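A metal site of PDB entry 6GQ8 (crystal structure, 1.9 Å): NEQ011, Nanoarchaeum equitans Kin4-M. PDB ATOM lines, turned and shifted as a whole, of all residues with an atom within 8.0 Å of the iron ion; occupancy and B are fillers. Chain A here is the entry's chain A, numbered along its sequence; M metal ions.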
ATOM      1  N   ASN A   7       9.122  11.442  13.625  1.00  0.00           N
ATOM      2  CA  ASN A   7       9.816  12.169  12.581  1.00  0.00           C
ATOM      3  C   ASN A   7       9.441  11.588  11.221  1.00  0.00           C
ATOM      4  O   ASN A   7       9.687  10.402  10.962  1.00  0.00           O
ATOM      5  CB  ASN A   7      11.330  12.112  12.794  1.00  0.00           C
ATOM      6  CG  ASN A   7      12.093  12.937  11.771  1.00  0.00           C
ATOM      7  OD1 ASN A   7      12.378  12.482  10.668  1.00  0.00           O
ATOM      8  ND2 ASN A   7      12.437  14.172  12.154  1.00  0.00           N
ATOM      9  N   LYS A   9      10.694  11.615   8.317  1.00  0.00           N
ATOM     10  CA  LYS A   9      11.760  11.078   7.480  1.00  0.00           C
ATOM     11  C   LYS A   9      12.441   9.872   8.098  1.00  0.00           C
ATOM     12  O   LYS A   9      13.000   9.042   7.362  1.00  0.00           O
ATOM     13  CB  LYS A   9      12.803  12.153   7.179  1.00  0.00           C
ATOM     14  CG  LYS A   9      12.434  13.096   6.042  1.00  0.00           C
ATOM     15  CD  LYS A   9      13.580  14.036   5.720  1.00  0.00           C
ATOM     16  CE  LYS A   9      13.290  14.866   4.479  1.00  0.00           C
ATOM     17  NZ  LYS A   9      14.424  15.748   4.116  1.00  0.00           N
ATOM     18  N   HIS A  10      12.435   9.746   9.422  1.00  0.00           N
ATOM     19  CA  HIS A  10      13.239   8.742  10.110  1.00  0.00           C
ATOM     20  C   HIS A  10      12.446   7.717  10.913  1.00  0.00           C
ATOM     21  O   HIS A  10      12.968   6.632  11.166  1.00  0.00           O
ATOM     22  CB  HIS A  10      14.242   9.412  11.056  1.00  0.00           C
ATOM     23  CG  HIS A  10      15.256  10.276  10.364  1.00  0.00           C
ATOM     24  ND1 HIS A  10      15.125  11.650  10.276  1.00  0.00           N
ATOM     25  CD2 HIS A  10      16.419   9.968   9.755  1.00  0.00           C
ATOM     26  CE1 HIS A  10      16.167  12.145   9.625  1.00  0.00           C
ATOM     27  NE2 HIS A  10      16.961  11.142   9.291  1.00  0.00           N
ATOM     28  N   VAL A  29      10.295   3.252   6.528  1.00  0.00           N
ATOM     29  CA  VAL A  29      10.893   4.487   7.002  1.00  0.00           C
ATOM     30  C   VAL A  29      10.762   5.532   5.905  1.00  0.00           C
ATOM     31  O   VAL A  29      11.097   5.260   4.745  1.00  0.00           O
ATOM     32  CB  VAL A  29      12.369   4.284   7.399  1.00  0.00           C
ATOM     33  CG1 VAL A  29      12.966   5.595   7.893  1.00  0.00           C
ATOM     34  CG2 VAL A  29      12.500   3.198   8.462  1.00  0.00           C
ATOM     35  N   HIS A  35      13.014   9.440   2.659  1.00  0.00           N
ATOM     36  CA  HIS A  35      14.347   9.727   3.179  1.00  0.00           C
ATOM     37  C   HIS A  35      15.371   9.525   2.062  1.00  0.00           C
ATOM     38  O   HIS A  35      15.212   8.624   1.229  1.00  0.00           O
ATOM     39  CB  HIS A  35      14.658   8.803   4.357  1.00  0.00           C
ATOM     40  CG  HIS A  35      15.943   9.135   5.065  1.00  0.00           C
ATOM     41  ND1 HIS A  35      17.164   8.618   4.668  1.00  0.00           N
ATOM     42  CD2 HIS A  35      16.194   9.890   6.155  1.00  0.00           C
ATOM     43  CE1 HIS A  35      18.111   9.065   5.482  1.00  0.00           C
ATOM     44  NE2 HIS A  35      17.550   9.836   6.390  1.00  0.00           N
ATOM     45  N   PRO A  36      16.414  10.357   2.014  1.00  0.00           N
ATOM     46  CA  PRO A  36      17.465  10.151   1.008  1.00  0.00           C
ATOM     47  C   PRO A  36      18.050   8.755   1.091  1.00  0.00           C
ATOM     48  O   PRO A  36      18.136   8.160   2.169  1.00  0.00           O
ATOM     49  CB  PRO A  36      18.505  11.222   1.353  1.00  0.00           C
ATOM     50  CG  PRO A  36      17.717  12.302   2.026  1.00  0.00           C
ATOM     51  CD  PRO A  36      16.612  11.596   2.779  1.00  0.00           C
ATOM     52  N   SER A  40      26.437   8.011   1.511  1.00  0.00           N
ATOM     53  CA  SER A  40      26.808   8.619   2.778  1.00  0.00           C
ATOM     54  C   SER A  40      25.610   9.031   3.630  1.00  0.00           C
ATOM     55  O   SER A  40      25.788   9.687   4.658  1.00  0.00           O
ATOM     56  CB  SER A  40      27.724   9.818   2.550  1.00  0.00           C
ATOM     57  OG  SER A  40      28.926   9.416   1.925  1.00  0.00           O
ATOM     58  N   HIS A  41      24.389   8.670   3.222  1.00  0.00           N
ATOM     59  CA  HIS A  41      23.195   9.028   3.982  1.00  0.00           C
ATOM     60  C   HIS A  41      22.058   8.117   3.543  1.00  0.00           C
ATOM     61  O   HIS A  41      21.508   8.306   2.459  1.00  0.00           O
ATOM     62  CB  HIS A  41      22.839  10.500   3.791  1.00  0.00           C
ATOM     63  CG  HIS A  41      21.727  10.969   4.676  1.00  0.00           C
ATOM     64  ND1 HIS A  41      21.028  12.138   4.452  1.00  0.00           N
ATOM     65  CD2 HIS A  41      21.203  10.434   5.807  1.00  0.00           C
ATOM     66  CE1 HIS A  41      20.122  12.301   5.396  1.00  0.00           C
ATOM     67  NE2 HIS A  41      20.210  11.279   6.234  1.00  0.00           N
ATOM     68  N   HIS A  42      21.705   7.152   4.390  1.00  0.00           N
ATOM     69  CA  HIS A  42      20.649   6.207   4.029  1.00  0.00           C
ATOM     70  C   HIS A  42      20.146   5.500   5.283  1.00  0.00           C
ATOM     71  O   HIS A  42      20.804   5.482   6.317  1.00  0.00           O
ATOM     72  CB  HIS A  42      21.131   5.180   3.007  1.00  0.00           C
ATOM     73  CG  HIS A  42      22.345   4.410   3.432  1.00  0.00           C
ATOM     74  ND1 HIS A  42      23.604   4.670   2.951  1.00  0.00           N
ATOM     75  CD2 HIS A  42      22.485   3.388   4.308  1.00  0.00           C
ATOM     76  CE1 HIS A  42      24.468   3.842   3.509  1.00  0.00           C
ATOM     77  NE2 HIS A  42      23.820   3.052   4.337  1.00  0.00           N
ATOM     78  N   ILE A  43      18.959   4.920   5.153  1.00  0.00           N
ATOM     79  CA  ILE A  43      18.415   4.048   6.193  1.00  0.00           C
ATOM     80  C   ILE A  43      19.019   2.668   5.984  1.00  0.00           C
ATOM     81  O   ILE A  43      18.795   2.041   4.938  1.00  0.00           O
ATOM     82  CB  ILE A  43      16.877   4.004   6.148  1.00  0.00           C
ATOM     83  CG1 ILE A  43      16.287   5.409   6.192  1.00  0.00           C
ATOM     84  CG2 ILE A  43      16.342   3.151   7.286  1.00  0.00           C
ATOM     85  CD1 ILE A  43      16.601   6.184   7.447  1.00  0.00           C
ATOM     86  N   TYR A  96      17.849   2.658  11.770  1.00  0.00           N
ATOM     87  CA  TYR A  96      19.125   3.352  11.875  1.00  0.00           C
ATOM     88  C   TYR A  96      19.393   4.130  10.606  1.00  0.00           C
ATOM     89  O   TYR A  96      19.326   3.587   9.509  1.00  0.00           O
ATOM     90  CB  TYR A  96      20.271   2.370  12.127  1.00  0.00           C
ATOM     91  CG  TYR A  96      21.643   3.008  12.075  1.00  0.00           C
ATOM     92  CD1 TYR A  96      22.077   3.858  13.090  1.00  0.00           C
ATOM     93  CD2 TYR A  96      22.518   2.751  11.029  1.00  0.00           C
ATOM     94  CE1 TYR A  96      23.331   4.440  13.057  1.00  0.00           C
ATOM     95  CE2 TYR A  96      23.771   3.333  10.982  1.00  0.00           C
ATOM     96  CZ  TYR A  96      24.172   4.177  12.000  1.00  0.00           C
ATOM     97  OH  TYR A  96      25.426   4.759  11.968  1.00  0.00           O
ATOM     98  N   CYS A  97      19.690   5.419  10.772  1.00  0.00           N
ATOM     99  CA  CYS A  97      20.153   6.279   9.690  1.00  0.00           C
ATOM    100  C   CYS A  97      21.637   6.563   9.884  1.00  0.00           C
ATOM    101  O   CYS A  97      22.081   6.798  11.011  1.00  0.00           O
ATOM    102  CB  CYS A  97      19.364   7.585   9.640  1.00  0.00           C
ATOM    103  SG  CYS A  97      20.060   8.831   8.543  1.00  0.00           S
ATOM    104  N   THR A  98      22.399   6.514   8.794  1.00  0.00           N
ATOM    105  CA  THR A  98      23.852   6.635   8.888  1.00  0.00           C
ATOM    106  C   THR A  98      24.299   8.015   9.351  1.00  0.00           C
ATOM    107  O   THR A  98      25.483   8.173   9.688  1.00  0.00           O
ATOM    108  CB  THR A  98      24.490   6.304   7.545  1.00  0.00           C
ATOM    109  OG1 THR A  98      23.958   7.148   6.524  1.00  0.00           O
ATOM    110  CG2 THR A  98      24.239   4.849   7.180  1.00  0.00           C
ATOM    111  N   LEU A  99      23.416   9.012   9.374  1.00  0.00           N
ATOM    112  CA  LEU A  99      23.769  10.336   9.853  1.00  0.00           C
ATOM    113  C   LEU A  99      22.996  10.775  11.085  1.00  0.00           C
ATOM    114  O   LEU A  99      23.531  11.550  11.880  1.00  0.00           O
ATOM    115  CB  LEU A  99      23.564  11.382   8.749  1.00  0.00           C
ATOM    116  CG  LEU A  99      24.505  11.340   7.543  1.00  0.00           C
ATOM    117  CD1 LEU A  99      24.249  12.541   6.632  1.00  0.00           C
ATOM    118  CD2 LEU A  99      25.950  11.313   7.989  1.00  0.00           C
ATOM    119  N   HIS A 100      21.760  10.312  11.263  1.00  0.00           N
ATOM    120  CA  HIS A 100      20.880  10.840  12.304  1.00  0.00           C
ATOM    121  C   HIS A 100      20.515   9.799  13.360  1.00  0.00           C
ATOM    122  O   HIS A 100      19.501   9.957  14.051  1.00  0.00           O
ATOM    123  CB  HIS A 100      19.638  11.462  11.671  1.00  0.00           C
ATOM    124  CG  HIS A 100      19.957  12.523  10.661  1.00  0.00           C
ATOM    125  ND1 HIS A 100      19.825  12.315   9.300  1.00  0.00           N
ATOM    126  CD2 HIS A 100      20.449  13.774  10.810  1.00  0.00           C
ATOM    127  CE1 HIS A 100      20.198  13.406   8.661  1.00  0.00           C
ATOM    128  NE2 HIS A 100      20.572  14.305   9.552  1.00  0.00           N
ATOM    129  N   GLY A 101      21.301   8.737  13.482  1.00  0.00           N
ATOM    130  CA  GLY A 101      21.180   7.869  14.634  1.00  0.00           C
ATOM    131  C   GLY A 101      20.005   6.908  14.547  1.00  0.00           C
ATOM    132  O   GLY A 101      19.563   6.502  13.466  1.00  0.00           O
ATOM    133  N   TRP A 103      16.075   5.460  15.712  1.00  0.00           N
ATOM    134  CA  TRP A 103      14.712   5.922  15.896  1.00  0.00           C
ATOM    135  C   TRP A 103      13.822   4.737  16.235  1.00  0.00           C
ATOM    136  O   TRP A 103      13.980   3.649  15.676  1.00  0.00           O
ATOM    137  CB  TRP A 103      14.197   6.633  14.634  1.00  0.00           C
ATOM    138  CG  TRP A 103      15.020   7.817  14.237  1.00  0.00           C
ATOM    139  CD1 TRP A 103      16.204   7.801  13.548  1.00  0.00           C
ATOM    140  CD2 TRP A 103      14.714   9.194  14.477  1.00  0.00           C
ATOM    141  NE1 TRP A 103      16.654   9.081  13.367  1.00  0.00           N
ATOM    142  CE2 TRP A 103      15.764   9.957  13.926  1.00  0.00           C
ATOM    143  CE3 TRP A 103      13.663   9.854  15.111  1.00  0.00           C
ATOM    144  CZ2 TRP A 103      15.782  11.350  13.987  1.00  0.00           C
ATOM    145  CZ3 TRP A 103      13.694  11.229  15.178  1.00  0.00           C
ATOM    146  CH2 TRP A 103      14.734  11.969  14.615  1.00  0.00           C
HETATM  147 FE    FE M   1      18.759  10.870   7.985  1.00  0.00          FE
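The iron ion is bound by a ring nitrogen (ND1) of His 100 (2.2 Å), a ring nitrogen (NE2) of His 10 (2.2 Å), a ring nitrogen (NE2) of His 35 (2.3 Å), a ring nitrogen (NE2) of His 41 (2.3 Å) and the side-chain sulfur (SG) of Cys 97 (2.5 Å).
O of His 100 sits at hydrogen-bond distance from NE1 of Trp 103, at 3.1 Å. The side-chain amide oxygen (OD1) of Asn 7 sits at hydrogen-bond distance from a ring nitrogen (ND1) of His 10 (2.9 Å). The backbone NH of Leu 99 lies close to the side-chain sulfur of Cys 97.
Five residues have an atom within 4 Å of the iron ion: His 10, His 35, His 41, Cys 97 and His 100.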
